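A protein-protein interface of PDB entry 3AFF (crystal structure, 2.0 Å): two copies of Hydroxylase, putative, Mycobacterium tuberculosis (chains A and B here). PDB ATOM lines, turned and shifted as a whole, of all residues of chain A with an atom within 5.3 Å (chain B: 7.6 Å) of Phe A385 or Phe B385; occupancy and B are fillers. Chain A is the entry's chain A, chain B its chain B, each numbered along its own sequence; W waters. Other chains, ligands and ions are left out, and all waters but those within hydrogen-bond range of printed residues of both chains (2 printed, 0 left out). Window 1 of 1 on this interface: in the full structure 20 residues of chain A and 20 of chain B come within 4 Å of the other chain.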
ATOM      1  N   PRO A 122      12.789  26.824  17.621  1.00  0.00           N
ATOM      2  CA  PRO A 122      12.979  25.480  17.124  1.00  0.00           C
ATOM      3  C   PRO A 122      11.619  24.848  16.690  1.00  0.00           C
ATOM      4  O   PRO A 122      11.008  24.156  17.472  1.00  0.00           O
ATOM      5  CB  PRO A 122      13.519  24.747  18.362  1.00  0.00           C
ATOM      6  CG  PRO A 122      12.880  25.441  19.505  1.00  0.00           C
ATOM      7  CD  PRO A 122      12.849  26.894  19.101  1.00  0.00           C
ATOM      8  N   PRO A 156      17.410  21.739  15.921  1.00  0.00           N
ATOM      9  CA  PRO A 156      18.504  20.840  16.183  1.00  0.00           C
ATOM     10  C   PRO A 156      18.837  20.067  14.896  1.00  0.00           C
ATOM     11  O   PRO A 156      18.002  19.969  14.030  1.00  0.00           O
ATOM     12  CB  PRO A 156      17.940  19.882  17.243  1.00  0.00           C
ATOM     13  CG  PRO A 156      16.414  19.921  17.027  1.00  0.00           C
ATOM     14  CD  PRO A 156      16.098  21.233  16.365  1.00  0.00           C
ATOM     15  N   PRO A 163      19.315  14.386  18.908  1.00  0.00           N
ATOM     16  CA  PRO A 163      19.996  15.689  18.702  1.00  0.00           C
ATOM     17  C   PRO A 163      21.473  15.672  19.002  1.00  0.00           C
ATOM     18  O   PRO A 163      21.912  15.136  20.012  1.00  0.00           O
ATOM     19  CB  PRO A 163      19.285  16.632  19.689  1.00  0.00           C
ATOM     20  CG  PRO A 163      17.923  15.999  19.916  1.00  0.00           C
ATOM     21  CD  PRO A 163      18.202  14.497  19.887  1.00  0.00           C
ATOM     22  N   ASP A 165      23.347  18.668  17.608  1.00  0.00           N
ATOM     23  CA  ASP A 165      23.771  20.084  17.359  1.00  0.00           C
ATOM     24  C   ASP A 165      22.507  20.932  17.214  1.00  0.00           C
ATOM     25  O   ASP A 165      21.402  20.389  17.155  1.00  0.00           O
ATOM     26  CB  ASP A 165      24.576  20.136  16.049  1.00  0.00           C
ATOM     27  CG  ASP A 165      25.538  21.351  15.972  1.00  0.00           C
ATOM     28  OD1 ASP A 165      25.451  22.329  16.747  1.00  0.00           O
ATOM     29  OD2 ASP A 165      26.398  21.307  15.105  1.00  0.00           O
ATOM     30  N   PHE A 166      22.662  22.252  17.128  1.00  0.00           N
ATOM     31  CA  PHE A 166      21.537  23.203  17.091  1.00  0.00           C
ATOM     32  C   PHE A 166      22.042  24.478  16.372  1.00  0.00           C
ATOM     33  O   PHE A 166      23.152  24.979  16.675  1.00  0.00           O
ATOM     34  CB  PHE A 166      21.041  23.572  18.500  1.00  0.00           C
ATOM     35  CG  PHE A 166      19.754  24.325  18.486  1.00  0.00           C
ATOM     36  CD1 PHE A 166      18.547  23.654  18.761  1.00  0.00           C
ATOM     37  CD2 PHE A 166      19.714  25.674  18.149  1.00  0.00           C
ATOM     38  CE1 PHE A 166      17.340  24.356  18.698  1.00  0.00           C
ATOM     39  CE2 PHE A 166      18.518  26.393  18.061  1.00  0.00           C
ATOM     40  CZ  PHE A 166      17.310  25.686  18.339  1.00  0.00           C
ATOM     41  N   TYR A 377      17.369  28.913  26.920  1.00  0.00           N
ATOM     42  CA  TYR A 377      18.655  28.313  26.498  1.00  0.00           C
ATOM     43  C   TYR A 377      19.810  28.708  27.409  1.00  0.00           C
ATOM     44  O   TYR A 377      20.715  27.955  27.676  1.00  0.00           O
ATOM     45  CB  TYR A 377      19.035  28.647  25.054  1.00  0.00           C
ATOM     46  CG  TYR A 377      18.081  28.227  23.982  1.00  0.00           C
ATOM     47  CD1 TYR A 377      17.013  27.313  24.229  1.00  0.00           C
ATOM     48  CD2 TYR A 377      18.269  28.701  22.681  1.00  0.00           C
ATOM     49  CE1 TYR A 377      16.133  26.956  23.192  1.00  0.00           C
ATOM     50  CE2 TYR A 377      17.404  28.355  21.680  1.00  0.00           C
ATOM     51  CZ  TYR A 377      16.343  27.500  21.932  1.00  0.00           C
ATOM     52  OH  TYR A 377      15.519  27.244  20.905  1.00  0.00           O
ATOM     53  N   PHE A 380      20.473  26.171  30.282  1.00  0.00           N
ATOM     54  CA  PHE A 380      21.049  24.858  29.929  1.00  0.00           C
ATOM     55  C   PHE A 380      22.588  24.802  30.060  1.00  0.00           C
ATOM     56  O   PHE A 380      23.307  25.591  29.425  1.00  0.00           O
ATOM     57  CB  PHE A 380      20.680  24.485  28.494  1.00  0.00           C
ATOM     58  CG  PHE A 380      19.225  24.137  28.288  1.00  0.00           C
ATOM     59  CD1 PHE A 380      18.530  23.360  29.206  1.00  0.00           C
ATOM     60  CD2 PHE A 380      18.568  24.573  27.143  1.00  0.00           C
ATOM     61  CE1 PHE A 380      17.213  22.994  28.973  1.00  0.00           C
ATOM     62  CE2 PHE A 380      17.268  24.247  26.898  1.00  0.00           C
ATOM     63  CZ  PHE A 380      16.569  23.459  27.830  1.00  0.00           C
ATOM     64  N   HIS A 383      24.452  20.678  27.111  1.00  0.00           N
ATOM     65  CA  HIS A 383      24.334  20.287  25.675  1.00  0.00           C
ATOM     66  C   HIS A 383      22.913  19.823  25.370  1.00  0.00           C
ATOM     67  O   HIS A 383      22.708  19.036  24.433  1.00  0.00           O
ATOM     68  CB  HIS A 383      25.338  19.136  25.340  1.00  0.00           C
ATOM     69  CG  HIS A 383      25.557  18.854  23.864  1.00  0.00           C
ATOM     70  ND1 HIS A 383      25.557  19.831  22.891  1.00  0.00           N
ATOM     71  CD2 HIS A 383      25.863  17.700  23.223  1.00  0.00           C
ATOM     72  CE1 HIS A 383      25.849  19.295  21.720  1.00  0.00           C
ATOM     73  NE2 HIS A 383      26.031  18.000  21.891  1.00  0.00           N
ATOM     74  N   GLU A 384      21.927  20.231  26.185  1.00  0.00           N
ATOM     75  CA  GLU A 384      20.532  19.832  25.963  1.00  0.00           C
ATOM     76  C   GLU A 384      20.119  20.180  24.571  1.00  0.00           C
ATOM     77  O   GLU A 384      20.313  21.298  24.100  1.00  0.00           O
ATOM     78  CB  GLU A 384      19.579  20.513  26.947  1.00  0.00           C
ATOM     79  CG  GLU A 384      19.626  19.845  28.313  1.00  0.00           C
ATOM     80  CD  GLU A 384      20.696  20.441  29.244  1.00  0.00           C
ATOM     81  OE1 GLU A 384      21.601  21.184  28.776  1.00  0.00           O
ATOM     82  OE2 GLU A 384      20.632  20.144  30.461  1.00  0.00           O
ATOM     83  N   PHE A 385      19.540  19.200  23.883  1.00  0.00           N
ATOM     84  CA  PHE A 385      19.082  19.398  22.494  1.00  0.00           C
ATOM     85  C   PHE A 385      20.098  19.843  21.432  1.00  0.00           C
ATOM     86  O   PHE A 385      19.702  20.413  20.407  1.00  0.00           O
ATOM     87  CB  PHE A 385      17.839  20.294  22.473  1.00  0.00           C
ATOM     88  CG  PHE A 385      16.834  19.929  23.513  1.00  0.00           C
ATOM     89  CD1 PHE A 385      16.023  18.788  23.361  1.00  0.00           C
ATOM     90  CD2 PHE A 385      16.638  20.769  24.629  1.00  0.00           C
ATOM     91  CE1 PHE A 385      15.076  18.466  24.361  1.00  0.00           C
ATOM     92  CE2 PHE A 385      15.740  20.487  25.583  1.00  0.00           C
ATOM     93  CZ  PHE A 385      14.928  19.332  25.482  1.00  0.00           C
ATOM     94  N   GLY A 386      21.390  19.579  21.661  1.00  0.00           N
ATOM     95  CA  GLY A 386      22.421  20.008  20.783  1.00  0.00           C
ATOM     96  C   GLY A 386      22.923  21.401  21.012  1.00  0.00           C
ATOM     97  O   GLY A 386      23.852  21.838  20.326  1.00  0.00           O
ATOM     98  N   LEU A 387      22.341  22.101  21.988  1.00  0.00           N
ATOM     99  CA  LEU A 387      22.658  23.497  22.267  1.00  0.00           C
ATOM    100  C   LEU A 387      24.077  23.644  22.866  1.00  0.00           C
ATOM    101  O   LEU A 387      24.603  22.684  23.481  1.00  0.00           O
ATOM    102  CB  LEU A 387      21.581  24.080  23.206  1.00  0.00           C
ATOM    103  CG  LEU A 387      20.312  24.524  22.468  1.00  0.00           C
ATOM    104  CD1 LEU A 387      19.055  24.570  23.388  1.00  0.00           C
ATOM    105  CD2 LEU A 387      20.514  25.842  21.713  1.00  0.00           C
ATOM    106  N   ALA B 121      17.011  13.455  31.999  1.00  0.00           N
ATOM    107  CA  ALA B 121      17.587  14.535  31.140  1.00  0.00           C
ATOM    108  C   ALA B 121      17.521  14.120  29.655  1.00  0.00           C
ATOM    109  O   ALA B 121      17.644  12.928  29.326  1.00  0.00           O
ATOM    110  CB  ALA B 121      19.019  14.862  31.525  1.00  0.00           C
ATOM    111  N   PRO B 122      17.340  15.107  28.753  1.00  0.00           N
ATOM    112  CA  PRO B 122      17.077  14.753  27.382  1.00  0.00           C
ATOM    113  C   PRO B 122      18.354  14.356  26.637  1.00  0.00           C
ATOM    114  O   PRO B 122      18.821  15.097  25.799  1.00  0.00           O
ATOM    115  CB  PRO B 122      16.494  16.039  26.808  1.00  0.00           C
ATOM    116  CG  PRO B 122      17.060  17.146  27.634  1.00  0.00           C
ATOM    117  CD  PRO B 122      17.415  16.575  28.961  1.00  0.00           C
ATOM    118  N   MET B 123      18.883  13.171  26.877  1.00  0.00           N
ATOM    119  CA  MET B 123      20.097  12.811  26.219  1.00  0.00           C
ATOM    120  C   MET B 123      19.829  11.753  25.122  1.00  0.00           C
ATOM    121  O   MET B 123      20.649  10.851  24.965  1.00  0.00           O
ATOM    122  CB  MET B 123      21.076  12.266  27.243  1.00  0.00           C
ATOM    123  CG  MET B 123      21.428  13.344  28.341  1.00  0.00           C
ATOM    124  SD  MET B 123      22.662  12.794  29.547  1.00  0.00           S
ATOM    125  CE  MET B 123      21.570  12.493  30.892  1.00  0.00           C
ATOM    126  N   GLY B 124      18.668  11.820  24.461  1.00  0.00           N
ATOM    127  CA  GLY B 124      18.322  10.888  23.387  1.00  0.00           C
ATOM    128  C   GLY B 124      16.952  11.293  22.931  1.00  0.00           C
ATOM    129  O   GLY B 124      16.428  12.343  23.388  1.00  0.00           O
ATOM    130  N   GLY B 154      14.426   9.980  29.504  1.00  0.00           N
ATOM    131  CA  GLY B 154      13.664  11.100  28.990  1.00  0.00           C
ATOM    132  C   GLY B 154      14.145  11.666  27.674  1.00  0.00           C
ATOM    133  O   GLY B 154      15.332  11.627  27.338  1.00  0.00           O
ATOM    134  N   GLY B 155      13.222  12.197  26.898  1.00  0.00           N
ATOM    135  CA  GLY B 155      13.623  12.812  25.656  1.00  0.00           C
ATOM    136  C   GLY B 155      12.393  13.191  24.861  1.00  0.00           C
ATOM    137  O   GLY B 155      11.258  12.831  25.205  1.00  0.00           O
ATOM    138  N   PRO B 156      12.606  13.907  23.761  1.00  0.00           N
ATOM    139  CA  PRO B 156      11.521  14.299  22.894  1.00  0.00           C
ATOM    140  C   PRO B 156      11.087  13.127  21.991  1.00  0.00           C
ATOM    141  O   PRO B 156      11.840  12.186  21.795  1.00  0.00           O
ATOM    142  CB  PRO B 156      12.156  15.397  22.054  1.00  0.00           C
ATOM    143  CG  PRO B 156      13.578  14.924  21.917  1.00  0.00           C
ATOM    144  CD  PRO B 156      13.921  14.381  23.254  1.00  0.00           C
ATOM    145  N   VAL B 157       9.848  13.215  21.496  1.00  0.00           N
ATOM    146  CA  VAL B 157       9.346  12.308  20.487  1.00  0.00           C
ATOM    147  C   VAL B 157       9.485  13.028  19.145  1.00  0.00           C
ATOM    148  O   VAL B 157       9.074  14.173  19.017  1.00  0.00           O
ATOM    149  CB  VAL B 157       7.827  11.977  20.751  1.00  0.00           C
ATOM    150  CG1 VAL B 157       7.225  11.236  19.527  1.00  0.00           C
ATOM    151  CG2 VAL B 157       7.675  11.188  22.002  1.00  0.00           C
ATOM    152  N   ILE B 158      10.077  12.379  18.170  1.00  0.00           N
ATOM    153  CA  ILE B 158      10.263  12.979  16.847  1.00  0.00           C
ATOM    154  C   ILE B 158       9.438  12.290  15.758  1.00  0.00           C
ATOM    155  O   ILE B 158       9.500  11.068  15.592  1.00  0.00           O
ATOM    156  CB  ILE B 158      11.761  13.079  16.529  1.00  0.00           C
ATOM    157  CG1 ILE B 158      12.380  14.067  17.571  1.00  0.00           C
ATOM    158  CG2 ILE B 158      11.984  13.527  15.060  1.00  0.00           C
ATOM    159  CD1 ILE B 158      13.851  14.189  17.532  1.00  0.00           C
ATOM    160  N   ARG B 162      10.387  16.181  13.028  1.00  0.00           N
ATOM    161  CA  ARG B 162      10.174  17.308  13.987  1.00  0.00           C
ATOM    162  C   ARG B 162       9.752  16.811  15.410  1.00  0.00           C
ATOM    163  O   ARG B 162       8.968  15.857  15.500  1.00  0.00           O
ATOM    164  CB  ARG B 162       9.067  18.214  13.418  1.00  0.00           C
ATOM    165  CG  ARG B 162       8.157  18.941  14.432  1.00  0.00           C
ATOM    166  CD  ARG B 162       7.459  20.173  13.808  1.00  0.00           C
ATOM    167  NE  ARG B 162       7.312  21.257  14.775  1.00  0.00           N
ATOM    168  CZ  ARG B 162       6.600  22.372  14.600  1.00  0.00           C
ATOM    169  NH1 ARG B 162       5.935  22.601  13.468  1.00  0.00           N
ATOM    170  NH2 ARG B 162       6.557  23.277  15.573  1.00  0.00           N
ATOM    171  N   PRO B 163      10.177  17.487  16.515  1.00  0.00           N
ATOM    172  CA  PRO B 163       9.607  17.142  17.861  1.00  0.00           C
ATOM    173  C   PRO B 163       8.101  17.430  18.029  1.00  0.00           C
ATOM    174  O   PRO B 163       7.642  18.537  17.676  1.00  0.00           O
ATOM    175  CB  PRO B 163      10.433  17.996  18.835  1.00  0.00           C
ATOM    176  CG  PRO B 163      11.710  18.343  18.085  1.00  0.00           C
ATOM    177  CD  PRO B 163      11.243  18.516  16.632  1.00  0.00           C
ATOM    178  N   VAL B 164       7.356  16.474  18.604  1.00  0.00           N
ATOM    179  CA  VAL B 164       5.924  16.584  18.733  1.00  0.00           C
ATOM    180  C   VAL B 164       5.518  16.285  20.163  1.00  0.00           C
ATOM    181  O   VAL B 164       4.380  16.533  20.560  1.00  0.00           O
ATOM    182  CB  VAL B 164       5.152  15.660  17.697  1.00  0.00           C
ATOM    183  CG1 VAL B 164       5.632  15.929  16.278  1.00  0.00           C
ATOM    184  CG2 VAL B 164       5.429  14.180  17.968  1.00  0.00           C
ATOM    185  N   ASP B 165       6.445  15.749  20.961  1.00  0.00           N
ATOM    186  CA  ASP B 165       6.072  15.387  22.299  1.00  0.00           C
ATOM    187  C   ASP B 165       7.371  15.210  23.069  1.00  0.00           C
ATOM    188  O   ASP B 165       8.460  15.172  22.485  1.00  0.00           O
ATOM    189  CB  ASP B 165       5.198  14.076  22.273  1.00  0.00           C
ATOM    190  CG  ASP B 165       4.270  13.918  23.485  1.00  0.00           C
ATOM    191  OD1 ASP B 165       4.363  14.638  24.484  1.00  0.00           O
ATOM    192  OD2 ASP B 165       3.430  12.985  23.490  1.00  0.00           O
ATOM    193  N   PHE B 166       7.224  15.106  24.375  1.00  0.00           N
ATOM    194  CA  PHE B 166       8.320  14.870  25.267  1.00  0.00           C
ATOM    195  C   PHE B 166       7.848  14.064  26.477  1.00  0.00           C
ATOM    196  O   PHE B 166       6.791  14.318  27.039  1.00  0.00           O
ATOM    197  CB  PHE B 166       8.862  16.260  25.740  1.00  0.00           C
ATOM    198  CG  PHE B 166      10.180  16.156  26.458  1.00  0.00           C
ATOM    199  CD1 PHE B 166      11.382  16.509  25.806  1.00  0.00           C
ATOM    200  CD2 PHE B 166      10.221  15.728  27.784  1.00  0.00           C
ATOM    201  CE1 PHE B 166      12.593  16.382  26.470  1.00  0.00           C
ATOM    202  CE2 PHE B 166      11.442  15.598  28.446  1.00  0.00           C
ATOM    203  CZ  PHE B 166      12.627  15.928  27.780  1.00  0.00           C
ATOM    204  N   GLY B 167       8.671  13.120  26.957  1.00  0.00           N
ATOM    205  CA  GLY B 167       8.233  12.395  28.152  1.00  0.00           C
ATOM    206  C   GLY B 167       9.205  11.349  28.569  1.00  0.00           C
ATOM    207  O   GLY B 167      10.403  11.486  28.313  1.00  0.00           O
ATOM    208  N   PRO B 373      17.799  20.374  33.880  1.00  0.00           N
ATOM    209  CA  PRO B 373      17.207  21.077  32.764  1.00  0.00           C
ATOM    210  C   PRO B 373      15.773  21.579  32.992  1.00  0.00           C
ATOM    211  O   PRO B 373      15.357  22.522  32.297  1.00  0.00           O
ATOM    212  CB  PRO B 373      17.312  20.056  31.616  1.00  0.00           C
ATOM    213  CG  PRO B 373      17.336  18.713  32.318  1.00  0.00           C
ATOM    214  CD  PRO B 373      18.196  19.009  33.506  1.00  0.00           C
ATOM    215  N   ALA B 376      14.917  25.178  33.145  1.00  0.00           N
ATOM    216  CA  ALA B 376      14.700  25.907  31.909  1.00  0.00           C
ATOM    217  C   ALA B 376      13.342  25.597  31.339  1.00  0.00           C
ATOM    218  O   ALA B 376      12.708  26.479  30.716  1.00  0.00           O
ATOM    219  CB  ALA B 376      15.764  25.561  30.923  1.00  0.00           C
ATOM    220  N   TYR B 377      12.878  24.343  31.517  1.00  0.00           N
ATOM    221  CA  TYR B 377      11.601  23.915  30.889  1.00  0.00           C
ATOM    222  C   TYR B 377      10.455  24.796  31.290  1.00  0.00           C
ATOM    223  O   TYR B 377       9.586  25.135  30.523  1.00  0.00           O
ATOM    224  CB  TYR B 377      11.199  22.469  31.220  1.00  0.00           C
ATOM    225  CG  TYR B 377      12.116  21.427  30.723  1.00  0.00           C
ATOM    226  CD1 TYR B 377      13.163  21.717  29.822  1.00  0.00           C
ATOM    227  CD2 TYR B 377      11.959  20.103  31.173  1.00  0.00           C
ATOM    228  CE1 TYR B 377      14.001  20.692  29.364  1.00  0.00           C
ATOM    229  CE2 TYR B 377      12.790  19.125  30.776  1.00  0.00           C
ATOM    230  CZ  TYR B 377      13.806  19.406  29.849  1.00  0.00           C
ATOM    231  OH  TYR B 377      14.599  18.350  29.513  1.00  0.00           O
ATOM    232  N   PHE B 380       9.719  27.694  28.955  1.00  0.00           N
ATOM    233  CA  PHE B 380       9.118  27.437  27.660  1.00  0.00           C
ATOM    234  C   PHE B 380       7.618  27.644  27.657  1.00  0.00           C
ATOM    235  O   PHE B 380       6.893  27.141  28.540  1.00  0.00           O
ATOM    236  CB  PHE B 380       9.485  26.051  27.101  1.00  0.00           C
ATOM    237  CG  PHE B 380      10.935  25.890  26.765  1.00  0.00           C
ATOM    238  CD1 PHE B 380      11.605  26.845  25.984  1.00  0.00           C
ATOM    239  CD2 PHE B 380      11.628  24.781  27.203  1.00  0.00           C
ATOM    240  CE1 PHE B 380      12.967  26.653  25.616  1.00  0.00           C
ATOM    241  CE2 PHE B 380      12.950  24.578  26.895  1.00  0.00           C
ATOM    242  CZ  PHE B 380      13.643  25.516  26.093  1.00  0.00           C
ATOM    243  N   ASN B 382       5.929  27.495  24.259  1.00  0.00           N
ATOM    244  CA  ASN B 382       5.541  27.367  22.881  1.00  0.00           C
ATOM    245  C   ASN B 382       5.837  25.988  22.336  1.00  0.00           C
ATOM    246  O   ASN B 382       6.170  25.854  21.151  1.00  0.00           O
ATOM    247  CB  ASN B 382       6.250  28.456  22.044  1.00  0.00           C
ATOM    248  CG  ASN B 382       5.679  29.853  22.310  1.00  0.00           C
ATOM    249  OD1 ASN B 382       6.242  30.620  23.055  1.00  0.00           O
ATOM    250  ND2 ASN B 382       4.557  30.138  21.744  1.00  0.00           N
ATOM    251  N   HIS B 383       5.803  24.993  23.224  1.00  0.00           N
ATOM    252  CA  HIS B 383       5.921  23.566  22.849  1.00  0.00           C
ATOM    253  C   HIS B 383       7.319  23.264  22.350  1.00  0.00           C
ATOM    254  O   HIS B 383       7.501  22.331  21.588  1.00  0.00           O
ATOM    255  CB  HIS B 383       4.875  23.257  21.757  1.00  0.00           C
ATOM    256  CG  HIS B 383       4.613  21.791  21.497  1.00  0.00           C
ATOM    257  ND1 HIS B 383       4.351  20.876  22.499  1.00  0.00           N
ATOM    258  CD2 HIS B 383       4.495  21.105  20.326  1.00  0.00           C
ATOM    259  CE1 HIS B 383       4.121  19.687  21.964  1.00  0.00           C
ATOM    260  NE2 HIS B 383       4.196  19.803  20.651  1.00  0.00           N
ATOM    261  N   GLU B 384       8.302  24.100  22.716  1.00  0.00           N
ATOM    262  CA  GLU B 384       9.709  23.827  22.314  1.00  0.00           C
ATOM    263  C   GLU B 384      10.111  22.352  22.640  1.00  0.00           C
ATOM    264  O   GLU B 384       9.874  21.869  23.760  1.00  0.00           O
ATOM    265  CB  GLU B 384      10.725  24.792  22.965  1.00  0.00           C
ATOM    266  CG  GLU B 384      10.635  26.201  22.451  1.00  0.00           C
ATOM    267  CD  GLU B 384       9.569  27.086  23.182  1.00  0.00           C
ATOM    268  OE1 GLU B 384       8.619  26.573  23.849  1.00  0.00           O
ATOM    269  OE2 GLU B 384       9.702  28.335  23.079  1.00  0.00           O
ATOM    270  N   PHE B 385      10.623  21.641  21.635  1.00  0.00           N
ATOM    271  CA  PHE B 385      11.109  20.265  21.777  1.00  0.00           C
ATOM    272  C   PHE B 385      10.056  19.268  22.241  1.00  0.00           C
ATOM    273  O   PHE B 385      10.374  18.254  22.876  1.00  0.00           O
ATOM    274  CB  PHE B 385      12.298  20.257  22.714  1.00  0.00           C
ATOM    275  CG  PHE B 385      13.348  21.278  22.338  1.00  0.00           C
ATOM    276  CD1 PHE B 385      14.049  21.161  21.147  1.00  0.00           C
ATOM    277  CD2 PHE B 385      13.609  22.391  23.168  1.00  0.00           C
ATOM    278  CE1 PHE B 385      15.015  22.064  20.805  1.00  0.00           C
ATOM    279  CE2 PHE B 385      14.586  23.316  22.807  1.00  0.00           C
ATOM    280  CZ  PHE B 385      15.297  23.167  21.644  1.00  0.00           C
ATOM    281  N   GLY B 386       8.789  19.581  21.965  1.00  0.00           N
ATOM    282  CA  GLY B 386       7.686  18.741  22.373  1.00  0.00           C
ATOM    283  C   GLY B 386       7.233  18.927  23.789  1.00  0.00           C
ATOM    284  O   GLY B 386       6.316  18.248  24.218  1.00  0.00           O
ATOM    285  N   LEU B 387       7.863  19.875  24.515  1.00  0.00           N
ATOM    286  CA  LEU B 387       7.529  20.152  25.928  1.00  0.00           C
ATOM    287  C   LEU B 387       6.139  20.794  26.146  1.00  0.00           C
ATOM    288  O   LEU B 387       5.602  21.442  25.248  1.00  0.00           O
ATOM    289  CB  LEU B 387       8.650  20.961  26.608  1.00  0.00           C
ATOM    290  CG  LEU B 387       9.965  20.206  26.887  1.00  0.00           C
ATOM    291  CD1 LEU B 387      11.165  21.148  26.951  1.00  0.00           C
ATOM    292  CD2 LEU B 387       9.862  19.293  28.139  1.00  0.00           C
ATOM    293  N   PRO B 388       5.528  20.563  27.329  1.00  0.00           N
ATOM    294  CA  PRO B 388       4.236  21.084  27.701  1.00  0.00           C
ATOM    295  C   PRO B 388       4.409  22.556  28.055  1.00  0.00           C
ATOM    296  O   PRO B 388       5.550  23.003  28.121  1.00  0.00           O
ATOM    297  CB  PRO B 388       3.858  20.291  28.965  1.00  0.00           C
ATOM    298  CG  PRO B 388       5.097  19.655  29.448  1.00  0.00           C
ATOM    299  CD  PRO B 388       6.119  19.688  28.361  1.00  0.00           C
HETATM  300  O   HOH W   1      10.477  22.055  18.890  1.00  0.00           O
HETATM  301  O   HOH W   2      19.822  16.444  23.955  1.00  0.00           O
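Among the printed residues, pairs that only touch across the chains: Glu A384 with Pro B373, Phe A380 with Ala B376, Phe A385 with Phe B385, Phe A385 with Pro B122, Phe A166 with Phe B385, Pro A122 with Glu B384, Glu A384 with Pro B122, Phe A380 with Pro B373, Phe A385 with Phe B166, Phe A380 with Phe B380, Pro A122 with Phe B385, Phe A380 with Tyr B377, Tyr A377 with Phe B385 and Tyr A377 with Phe B380.
The backbone NH (N) of Phe A166 lies within hydrogen-bond range of the backbone carbonyl oxygen (O) of Gly A386, at 3.4 Å.
OE1 of Glu B384 sits at hydrogen-bond distance from N of Asn B382, at 2.9 Å.
N of Phe B166 is in hydrogen-bond range of O of Gly B386 (3.3 Å).
Pro A122 touches Phe B385, and with the chains exchanged Phe A385 touches Pro B122.
Phe A166 touches Phe B385, and with the chains exchanged Phe A385 touches Phe B166.
Tyr A377 touches Phe B380, and with the chains exchanged Phe A380 touches Tyr B377.
Phe A380 touches its own counterpart, Phe B380.
Positions printed for both chains: 122, 156, 163, 165, 166, 377, 380, 383, 384, 385, 386 and 387.
Of the 14 pairs that touch across the chains among the printed residues, 10 have their exchanged pair printed and touching as well.
Of the printed residues of chain B, Pro A122 touches Glu B384 (3.8 Å) and Phe B385 (3.9 Å).
Pro A163 touches none of the printed residues of chain B.
Of the printed residues of chain B, Phe A385 touches Pro B122, Phe B166 and Phe B385.
Of the printed residues of chain A, Pro B122 touches Glu A384 (3.8 Å) and Phe A385 (3.7 Å).
Printed residues of chain A within 4 Å of Phe B166: Phe A385 (3.9 Å).
Printed residues of chain A within 4 Å of Pro B373: Phe A380 (3.8 Å) and Glu A384 (3.5 Å).
Of the printed residues of chain A, Tyr B377 touches Phe A380.
His B383 touches none of the printed residues of chain A.
Of the printed residues of chain A, Phe B385 touches Pro A122, Phe A166, Tyr A377 and Phe A385.
The nearest residue of chain B that does not touch Phe A385 is Tyr B377 (4.2 Å).
The nearest printed residue of chain A that does not touch Pro B373 is Phe A385 (6.2 Å).
Of the 12 printed residues of chain A, 6 touch a printed residue of chain B.
Printed residues of chain A that touch a printed residue of chain B: Pro A122, Phe A166, Tyr A377, Phe A380, Glu A384 and Phe A385.
Hydrophobic or aromatic side chains of chain A that line the printed part of chain B: Pro A122, Phe A166, Tyr A377, Phe A380 and Phe A385.
Hydrophobic or aromatic side chains of chain B within 4 Å of the printed part of chain A: Pro B122, Phe B166, Pro B373, Ala B376, Tyr B377, Phe B380 and Phe B385.
Among the printed residues, 14 pairs touch across the chains.
Water W2 lies within hydrogen-bond range of O of Pro B122 (2.5 Å) and N of Phe A385 (2.8 Å).
Water W1 bridges the backbone carbonyl oxygen (O) of Pro A122 and the backbone NH (N) of Phe B385.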
